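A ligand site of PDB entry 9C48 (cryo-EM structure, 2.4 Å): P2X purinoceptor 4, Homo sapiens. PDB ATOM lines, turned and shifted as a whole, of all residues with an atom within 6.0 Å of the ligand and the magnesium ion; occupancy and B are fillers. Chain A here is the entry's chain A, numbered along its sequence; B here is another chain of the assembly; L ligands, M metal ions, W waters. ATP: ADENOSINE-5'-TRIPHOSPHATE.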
ATOM      1  N   THR A 139      19.300 -14.187  33.149  1.00  0.00           N
ATOM      2  CA  THR A 139      20.253 -13.841  32.100  1.00  0.00           C
ATOM      3  C   THR A 139      19.866 -12.545  31.402  1.00  0.00           C
ATOM      4  O   THR A 139      20.747 -11.752  31.038  1.00  0.00           O
ATOM      5  CB  THR A 139      20.357 -14.990  31.090  1.00  0.00           C
ATOM      6  OG1 THR A 139      21.034 -14.533  29.909  1.00  0.00           O
ATOM      7  CG2 THR A 139      18.975 -15.516  30.719  1.00  0.00           C
ATOM      8  N   HIS A 140      18.577 -12.293  31.227  1.00  0.00           N
ATOM      9  CA  HIS A 140      18.107 -11.103  30.530  1.00  0.00           C
ATOM     10  C   HIS A 140      17.809  -9.944  31.469  1.00  0.00           C
ATOM     11  O   HIS A 140      17.413  -8.873  31.003  1.00  0.00           O
ATOM     12  CB  HIS A 140      16.857 -11.426  29.703  1.00  0.00           C
ATOM     13  CG  HIS A 140      17.054 -12.545  28.724  1.00  0.00           C
ATOM     14  ND1 HIS A 140      17.703 -12.364  27.517  1.00  0.00           N
ATOM     15  CD2 HIS A 140      16.704 -13.844  28.772  1.00  0.00           C
ATOM     16  CE1 HIS A 140      17.736 -13.509  26.873  1.00  0.00           C
ATOM     17  NE2 HIS A 140      17.137 -14.432  27.611  1.00  0.00           N
ATOM     18  N   GLU A 168      18.092   0.913  30.616  1.00  0.00           N
ATOM     19  CA  GLU A 168      18.026   1.233  29.203  1.00  0.00           C
ATOM     20  C   GLU A 168      16.688   0.794  28.605  1.00  0.00           C
ATOM     21  O   GLU A 168      16.152  -0.262  28.938  1.00  0.00           O
ATOM     22  CB  GLU A 168      19.170   0.545  28.462  1.00  0.00           C
ATOM     23  CG  GLU A 168      19.129   0.684  26.956  1.00  0.00           C
ATOM     24  CD  GLU A 168      20.126  -0.229  26.276  1.00  0.00           C
ATOM     25  OE1 GLU A 168      21.161   0.269  25.782  1.00  0.00           O
ATOM     26  OE2 GLU A 168      19.892  -1.454  26.227  1.00  0.00           O
ATOM     27  N   ASP A 170      15.377   0.055  24.941  1.00  0.00           N
ATOM     28  CA  ASP A 170      15.810  -0.159  23.570  1.00  0.00           C
ATOM     29  C   ASP A 170      14.707  -0.764  22.710  1.00  0.00           C
ATOM     30  O   ASP A 170      14.994  -1.475  21.747  1.00  0.00           O
ATOM     31  CB  ASP A 170      17.061  -1.045  23.537  1.00  0.00           C
ATOM     32  CG  ASP A 170      16.827  -2.396  24.164  1.00  0.00           C
ATOM     33  OD1 ASP A 170      15.810  -2.570  24.868  1.00  0.00           O
ATOM     34  OD2 ASP A 170      17.660  -3.294  23.950  1.00  0.00           O
ATOM     35  N   VAL A 288      15.471 -14.052  13.492  1.00  0.00           N
ATOM     36  CA  VAL A 288      16.110 -14.372  14.763  1.00  0.00           C
ATOM     37  C   VAL A 288      17.522 -13.785  14.753  1.00  0.00           C
ATOM     38  O   VAL A 288      18.330 -14.122  13.883  1.00  0.00           O
ATOM     39  CB  VAL A 288      16.152 -15.894  14.998  1.00  0.00           C
ATOM     40  CG1 VAL A 288      16.954 -16.212  16.248  1.00  0.00           C
ATOM     41  CG2 VAL A 288      14.746 -16.438  15.123  1.00  0.00           C
ATOM     42  N   SER A 289      17.790 -12.916  15.716  1.00  0.00           N
ATOM     43  CA  SER A 289      19.103 -12.296  15.891  1.00  0.00           C
ATOM     44  C   SER A 289      19.605 -11.581  14.630  1.00  0.00           C
ATOM     45  O   SER A 289      20.585 -12.023  14.011  1.00  0.00           O
ATOM     46  CB  SER A 289      20.118 -13.327  16.366  1.00  0.00           C
ATOM     47  OG  SER A 289      21.328 -12.708  16.751  1.00  0.00           O
ATOM     48  N   PRO A 290      18.965 -10.492  14.228  1.00  0.00           N
ATOM     49  CA  PRO A 290      19.403  -9.778  13.027  1.00  0.00           C
ATOM     50  C   PRO A 290      20.451  -8.706  13.323  1.00  0.00           C
ATOM     51  O   PRO A 290      20.623  -8.261  14.454  1.00  0.00           O
ATOM     52  CB  PRO A 290      18.097  -9.133  12.529  1.00  0.00           C
ATOM     53  CG  PRO A 290      17.354  -8.845  13.786  1.00  0.00           C
ATOM     54  CD  PRO A 290      17.751  -9.894  14.806  1.00  0.00           C
ATOM     55  N   ASN A 293      25.207  -5.632  16.931  1.00  0.00           N
ATOM     56  CA  ASN A 293      25.233  -4.553  17.916  1.00  0.00           C
ATOM     57  C   ASN A 293      25.977  -5.002  19.159  1.00  0.00           C
ATOM     58  O   ASN A 293      26.203  -6.185  19.386  1.00  0.00           O
ATOM     59  CB  ASN A 293      23.816  -4.086  18.267  1.00  0.00           C
ATOM     60  CG  ASN A 293      22.994  -5.151  18.965  1.00  0.00           C
ATOM     61  OD1 ASN A 293      23.192  -5.430  20.143  1.00  0.00           O
ATOM     62  ND2 ASN A 293      22.053  -5.736  18.242  1.00  0.00           N
ATOM     63  N   ARG A 295      27.254  -3.128  23.381  1.00  0.00           N
ATOM     64  CA  ARG A 295      27.096  -2.068  24.367  1.00  0.00           C
ATOM     65  C   ARG A 295      28.435  -1.664  24.944  1.00  0.00           C
ATOM     66  O   ARG A 295      29.289  -2.518  25.214  1.00  0.00           O
ATOM     67  CB  ARG A 295      26.163  -2.493  25.506  1.00  0.00           C
ATOM     68  CG  ARG A 295      24.688  -2.535  25.150  1.00  0.00           C
ATOM     69  CD  ARG A 295      23.883  -3.078  26.307  1.00  0.00           C
ATOM     70  NE  ARG A 295      22.459  -3.149  26.006  1.00  0.00           N
ATOM     71  CZ  ARG A 295      21.854  -4.198  25.456  1.00  0.00           C
ATOM     72  NH1 ARG A 295      22.537  -5.271  25.089  1.00  0.00           N
ATOM     73  NH2 ARG A 295      20.539  -4.161  25.261  1.00  0.00           N
ATOM     74  N   LYS A 313      24.216   1.800  23.287  1.00  0.00           N
ATOM     75  CA  LYS A 313      23.947   0.584  22.481  1.00  0.00           C
ATOM     76  C   LYS A 313      24.250   0.988  21.039  1.00  0.00           C
ATOM     77  O   LYS A 313      23.553   1.874  20.523  1.00  0.00           O
ATOM     78  CB  LYS A 313      22.529   0.039  22.669  1.00  0.00           C
ATOM     79  CG  LYS A 313      22.304  -1.319  22.010  1.00  0.00           C
ATOM     80  CD  LYS A 313      20.951  -1.938  22.284  1.00  0.00           C
ATOM     81  CE  LYS A 313      20.848  -3.341  21.714  1.00  0.00           C
ATOM     82  NZ  LYS A 313      19.493  -3.914  21.895  1.00  0.00           N
ATOM     83  N   TYR A 315      24.642   0.154  17.014  1.00  0.00           N
ATOM     84  CA  TYR A 315      24.408  -0.636  15.814  1.00  0.00           C
ATOM     85  C   TYR A 315      25.333  -0.125  14.728  1.00  0.00           C
ATOM     86  O   TYR A 315      25.605   1.075  14.641  1.00  0.00           O
ATOM     87  CB  TYR A 315      22.954  -0.542  15.343  1.00  0.00           C
ATOM     88  CG  TYR A 315      21.908  -0.867  16.376  1.00  0.00           C
ATOM     89  CD1 TYR A 315      21.558   0.044  17.362  1.00  0.00           C
ATOM     90  CD2 TYR A 315      21.255  -2.090  16.361  1.00  0.00           C
ATOM     91  CE1 TYR A 315      20.599  -0.260  18.303  1.00  0.00           C
ATOM     92  CE2 TYR A 315      20.290  -2.406  17.299  1.00  0.00           C
ATOM     93  CZ  TYR A 315      19.961  -1.484  18.262  1.00  0.00           C
ATOM     94  OH  TYR A 315      19.005  -1.795  19.198  1.00  0.00           O
ATOM     95  N   LYS B  67      28.280 -12.270  22.452  1.00  0.00           N
ATOM     96  CA  LYS B  67      27.580 -11.397  23.398  1.00  0.00           C
ATOM     97  C   LYS B  67      27.442 -12.121  24.729  1.00  0.00           C
ATOM     98  O   LYS B  67      27.085 -13.299  24.755  1.00  0.00           O
ATOM     99  CB  LYS B  67      26.208 -10.985  22.871  1.00  0.00           C
ATOM    100  CG  LYS B  67      25.431 -10.085  23.819  1.00  0.00           C
ATOM    101  CD  LYS B  67      24.132  -9.601  23.212  1.00  0.00           C
ATOM    102  CE  LYS B  67      24.343  -8.376  22.355  1.00  0.00           C
ATOM    103  NZ  LYS B  67      23.077  -7.826  21.844  1.00  0.00           N
ATOM    104  N   VAL B  68      27.723 -11.415  25.821  1.00  0.00           N
ATOM    105  CA  VAL B  68      27.690 -11.976  27.170  1.00  0.00           C
ATOM    106  C   VAL B  68      26.578 -11.297  27.950  1.00  0.00           C
ATOM    107  O   VAL B  68      26.360 -10.090  27.813  1.00  0.00           O
ATOM    108  CB  VAL B  68      29.053 -11.814  27.878  1.00  0.00           C
ATOM    109  CG1 VAL B  68      29.056 -12.523  29.212  1.00  0.00           C
ATOM    110  CG2 VAL B  68      30.159 -12.323  26.995  1.00  0.00           C
ATOM    111  N   LYS B  69      25.873 -12.077  28.765  1.00  0.00           N
ATOM    112  CA  LYS B  69      24.840 -11.562  29.653  1.00  0.00           C
ATOM    113  C   LYS B  69      25.094 -12.048  31.068  1.00  0.00           C
ATOM    114  O   LYS B  69      25.567 -13.165  31.275  1.00  0.00           O
ATOM    115  CB  LYS B  69      23.441 -11.973  29.197  1.00  0.00           C
ATOM    116  CG  LYS B  69      22.962 -11.238  27.977  1.00  0.00           C
ATOM    117  CD  LYS B  69      21.463 -11.305  27.841  1.00  0.00           C
ATOM    118  CE  LYS B  69      21.010 -10.527  26.627  1.00  0.00           C
ATOM    119  NZ  LYS B  69      21.611  -9.166  26.596  1.00  0.00           N
ATOM    120  N   THR B 186      26.214 -16.187  30.741  1.00  0.00           N
ATOM    121  CA  THR B 186      25.957 -16.936  29.513  1.00  0.00           C
ATOM    122  C   THR B 186      26.553 -16.210  28.325  1.00  0.00           C
ATOM    123  O   THR B 186      26.624 -14.980  28.305  1.00  0.00           O
ATOM    124  CB  THR B 186      24.449 -17.162  29.294  1.00  0.00           C
ATOM    125  OG1 THR B 186      23.752 -15.921  29.441  1.00  0.00           O
ATOM    126  CG2 THR B 186      23.922 -18.151  30.310  1.00  0.00           C
ATOM    127  N   LEU B 187      27.000 -16.973  27.341  1.00  0.00           N
ATOM    128  CA  LEU B 187      27.671 -16.443  26.165  1.00  0.00           C
ATOM    129  C   LEU B 187      26.976 -16.954  24.913  1.00  0.00           C
ATOM    130  O   LEU B 187      26.763 -18.151  24.770  1.00  0.00           O
ATOM    131  CB  LEU B 187      29.156 -16.835  26.146  1.00  0.00           C
ATOM    132  CG  LEU B 187      29.939 -16.687  24.850  1.00  0.00           C
ATOM    133  CD1 LEU B 187      30.135 -15.217  24.508  1.00  0.00           C
ATOM    134  CD2 LEU B 187      31.270 -17.413  24.929  1.00  0.00           C
ATOM    135  N   LEU B 188      26.631 -16.036  24.012  1.00  0.00           N
ATOM    136  CA  LEU B 188      26.059 -16.387  22.720  1.00  0.00           C
ATOM    137  C   LEU B 188      27.130 -16.271  21.645  1.00  0.00           C
ATOM    138  O   LEU B 188      27.805 -15.243  21.535  1.00  0.00           O
ATOM    139  CB  LEU B 188      24.879 -15.464  22.385  1.00  0.00           C
ATOM    140  CG  LEU B 188      24.437 -15.411  20.915  1.00  0.00           C
ATOM    141  CD1 LEU B 188      23.791 -16.718  20.493  1.00  0.00           C
ATOM    142  CD2 LEU B 188      23.513 -14.244  20.669  1.00  0.00           C
ATOM    143  N   LYS B 190      27.736 -16.407  17.616  1.00  0.00           N
ATOM    144  CA  LYS B 190      27.139 -16.338  16.281  1.00  0.00           C
ATOM    145  C   LYS B 190      28.249 -16.555  15.261  1.00  0.00           C
ATOM    146  O   LYS B 190      29.161 -15.722  15.141  1.00  0.00           O
ATOM    147  CB  LYS B 190      26.442 -15.003  16.060  1.00  0.00           C
ATOM    148  CG  LYS B 190      25.218 -14.793  16.928  1.00  0.00           C
ATOM    149  CD  LYS B 190      24.674 -13.385  16.773  1.00  0.00           C
ATOM    150  CE  LYS B 190      24.372 -13.044  15.325  1.00  0.00           C
ATOM    151  NZ  LYS B 190      23.795 -11.690  15.191  1.00  0.00           N
ATOM    152  N   THR B 211      12.809 -17.594  18.312  1.00  0.00           N
ATOM    153  CA  THR B 211      13.153 -16.625  19.344  1.00  0.00           C
ATOM    154  C   THR B 211      12.775 -17.117  20.736  1.00  0.00           C
ATOM    155  O   THR B 211      13.518 -16.905  21.704  1.00  0.00           O
ATOM    156  CB  THR B 211      12.466 -15.281  19.066  1.00  0.00           C
ATOM    157  OG1 THR B 211      11.059 -15.495  18.903  1.00  0.00           O
ATOM    158  CG2 THR B 211      13.033 -14.634  17.801  1.00  0.00           C
ATOM    159  N   LEU B 214      15.440 -19.570  21.699  1.00  0.00           N
ATOM    160  CA  LEU B 214      16.711 -18.904  21.931  1.00  0.00           C
ATOM    161  C   LEU B 214      16.712 -18.071  23.202  1.00  0.00           C
ATOM    162  O   LEU B 214      17.788 -17.784  23.740  1.00  0.00           O
ATOM    163  CB  LEU B 214      17.071 -18.035  20.737  1.00  0.00           C
ATOM    164  CG  LEU B 214      18.540 -17.605  20.597  1.00  0.00           C
ATOM    165  CD1 LEU B 214      19.438 -18.828  20.424  1.00  0.00           C
ATOM    166  CD2 LEU B 214      18.725 -16.642  19.448  1.00  0.00           C
ATOM    167  N   LYS B 215      15.544 -17.664  23.692  1.00  0.00           N
ATOM    168  CA  LYS B 215      15.505 -16.816  24.878  1.00  0.00           C
ATOM    169  C   LYS B 215      15.826 -17.579  26.155  1.00  0.00           C
ATOM    170  O   LYS B 215      16.225 -16.968  27.148  1.00  0.00           O
ATOM    171  CB  LYS B 215      14.129 -16.155  24.998  1.00  0.00           C
ATOM    172  CG  LYS B 215      14.037 -14.779  24.363  1.00  0.00           C
ATOM    173  CD  LYS B 215      13.119 -13.871  25.145  1.00  0.00           C
ATOM    174  CE  LYS B 215      13.913 -12.923  26.031  1.00  0.00           C
ATOM    175  NZ  LYS B 215      14.764 -12.013  25.225  1.00  0.00           N
ATOM    176  N   ILE B 229      24.058 -20.873  22.946  1.00  0.00           N
ATOM    177  CA  ILE B 229      24.275 -20.132  24.185  1.00  0.00           C
ATOM    178  C   ILE B 229      24.913 -21.075  25.199  1.00  0.00           C
ATOM    179  O   ILE B 229      24.345 -22.118  25.536  1.00  0.00           O
ATOM    180  CB  ILE B 229      22.964 -19.542  24.719  1.00  0.00           C
ATOM    181  CG1 ILE B 229      22.322 -18.641  23.657  1.00  0.00           C
ATOM    182  CG2 ILE B 229      23.207 -18.770  26.012  1.00  0.00           C
ATOM    183  CD1 ILE B 229      21.037 -18.005  24.076  1.00  0.00           C
HETATM  184  PG  ATP L   1      19.562  -7.763  23.699  1.00  0.00           P
HETATM  185  O1G ATP L   1      18.793  -8.432  24.813  1.00  0.00           O
HETATM  186  O2G ATP L   1      18.932  -6.437  23.316  1.00  0.00           O
HETATM  187  O3G ATP L   1      21.026  -7.580  24.089  1.00  0.00           O
HETATM  188  PB  ATP L   1      19.095  -8.102  20.954  1.00  0.00           P
HETATM  189  O1B ATP L   1      17.716  -7.547  21.057  1.00  0.00           O
HETATM  190  O2B ATP L   1      20.054  -7.063  20.442  1.00  0.00           O
HETATM  191  O3B ATP L   1      19.576  -8.688  22.352  1.00  0.00           O
HETATM  192  PA  ATP L   1      20.435 -10.223  19.765  1.00  0.00           P
HETATM  193  O1A ATP L   1      20.765 -10.201  18.303  1.00  0.00           O
HETATM  194  O2A ATP L   1      21.555  -9.627  20.527  1.00  0.00           O
HETATM  195  O3A ATP L   1      19.098  -9.386  20.009  1.00  0.00           O
HETATM  196  O5' ATP L   1      20.224 -11.714  20.228  1.00  0.00           O
HETATM  197  C5' ATP L   1      18.964 -12.355  19.934  1.00  0.00           C
HETATM  198  C4' ATP L   1      18.383 -12.903  21.252  1.00  0.00           C
HETATM  199  O4' ATP L   1      19.406 -13.619  21.994  1.00  0.00           O
HETATM  200  C3' ATP L   1      17.922 -11.723  22.184  1.00  0.00           C
HETATM  201  O3' ATP L   1      16.603 -11.967  22.660  1.00  0.00           O
HETATM  202  C2' ATP L   1      18.912 -11.751  23.353  1.00  0.00           C
HETATM  203  O2' ATP L   1      18.237 -11.472  24.582  1.00  0.00           O
HETATM  204  C1' ATP L   1      19.445 -13.169  23.334  1.00  0.00           C
HETATM  205  N9  ATP L   1      20.855 -13.189  23.810  1.00  0.00           N
HETATM  206  C8  ATP L   1      21.874 -12.512  23.266  1.00  0.00           C
HETATM  207  N7  ATP L   1      23.043 -12.705  23.901  1.00  0.00           N
HETATM  208  C5  ATP L   1      22.720 -13.553  24.902  1.00  0.00           C
HETATM  209  C6  ATP L   1      23.441 -14.190  25.976  1.00  0.00           C
HETATM  210  N6  ATP L   1      24.757 -13.984  26.145  1.00  0.00           N
HETATM  211  N1  ATP L   1      22.732 -15.019  26.834  1.00  0.00           N
HETATM  212  C2  ATP L   1      21.434 -15.206  26.647  1.00  0.00           C
HETATM  213  N3  ATP L   1      20.670 -14.675  25.708  1.00  0.00           N
HETATM  214  C4  ATP L   1      21.327 -13.863  24.851  1.00  0.00           C
HETATM  215 MG    MG M   1      16.713  -5.466  24.043  1.00  0.00          MG
HETATM  216  O   HOH W   1      15.218  -8.869  21.694  1.00  0.00           O
HETATM  217  O   HOH W   2      21.964  -8.858  16.418  1.00  0.00           O
HETATM  218  O   HOH W   3      16.789  -5.478  27.497  1.00  0.00           O
HETATM  219  O   HOH W   4      15.767  -9.221  24.749  1.00  0.00           O
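O2A of the ligand is in salt-bridge range of NZ of Lys 67 of chain B (2.7 Å).
NZ of Lys 313 is in salt-bridge range of O2B of the ligand (3.5 Å).
OG of Ser 289 sits at hydrogen-bond distance from O1A of the ligand (3.0 Å).
A ring nitrogen (ND1) of His 140 lies close to an oxygen (O2') of the ligand.
O3' of the ligand sits at hydrogen-bond distance from NZ of Lys 215 of chain B (3.2 Å).
The side-chain amide nitrogen (ND2) of Asn 293 lies within hydrogen-bond range of an oxygen (O2B) of the ligand, 3.3 Å away.
An oxygen (O3G) of the ligand is in salt-bridge range of the side-chain amino group (NZ) of Lys 69 of chain B (3.0 Å).
The guanidinium group (NH1) of Arg 295 lies within salt-bridge range of an oxygen (O3G) of the ligand (2.9 Å).
O of Lys 67 of chain B lies within hydrogen-bond range of N6 of the ligand, 2.8 Å away.
O of Thr 186 of chain B sits at hydrogen-bond distance from N6 of the ligand (3.0 Å).
A nitrogen (N1) of the ligand lies within hydrogen-bond range of the side-chain hydroxyl (OG1) of Thr 186 of chain B (2.9 Å).
The side-chain hydroxyl (OG) of Ser 289 lies within hydrogen-bond range of the side-chain amino group (NZ) of Lys 190 of chain B.
The backbone carbonyl oxygen of Lys 215 of chain B sits at hydrogen-bond distance from a ring nitrogen (NE2) of His 140, 2.7 Å away.
The side-chain carboxylate (OE2) of Glu 168 lies within salt-bridge range of the guanidinium group (NH2) of Arg 295.
The side-chain carboxylate of Asp 170 lies close to the guanidinium group of Arg 295, 3.3 Å away.
The side-chain hydroxyl (OH) of Tyr 315 lies within hydrogen-bond range of the side-chain amino group (NZ) of Lys 313 (3.5 Å).
OD2 of Asp 170 lies close to NZ of Lys 313, at 2.8 Å.
The backbone carbonyl oxygen (O) of Thr 186 of chain B is in hydrogen-bond range of the backbone NH (N) of Lys 69 of chain B, 3.0 Å away.
NZ of Lys 67 of chain B is in hydrogen-bond range of OD1 of Asn 293.
OG1 of Thr 139 touches C2 of the ligand, at 3.4 Å.
CA of Val 68 of chain B touches N6 of the ligand, 3.7 Å away.
Leu 187 of chain B touches the ligand.
Leu 188 of chain B touches the ligand.
Ile 229 of chain B touches the ligand.
15 residues have an atom within 4 Å of the ligand: Thr 139, His 140, Asp 170, Ser 289, Asn 293, Arg 295, Lys 313, Lys 67 of chain B, Val 68 of chain B, Lys 69 of chain B, Thr 186 of chain B, Leu 187 of chain B, Leu 188 of chain B, Lys 215 of chain B and Ile 229 of chain B.
The nearest printed residue that does not touch the ligand is Leu 214 of chain B (4.01 Å).
Merely in contact with the magnesium ion: Lys 313 (3.8 Å).
Two residues have an atom within 4 Å of the magnesium ion: Asp 170 and Lys 313.
Along chain A the residues within 4 Å of the magnesium ion span positions 170 to 313.
The nearest printed residue that does not touch the magnesium ion is Arg 295 (4.2 Å).
The magnesium ion is bound by OD2 of Asp 170 and O2G of the ligand.
The magnesium ion has two donor atoms within binding distance.
Water W2 lies within hydrogen-bond range of O of Pro 290 (2.5 Å) and O1A of the ligand (2.6 Å).
Water W4 bridges the side-chain amino group of Lys 215 of chain B (3.0 Å) and an oxygen (O1G) of the ligand (3.1 Å).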
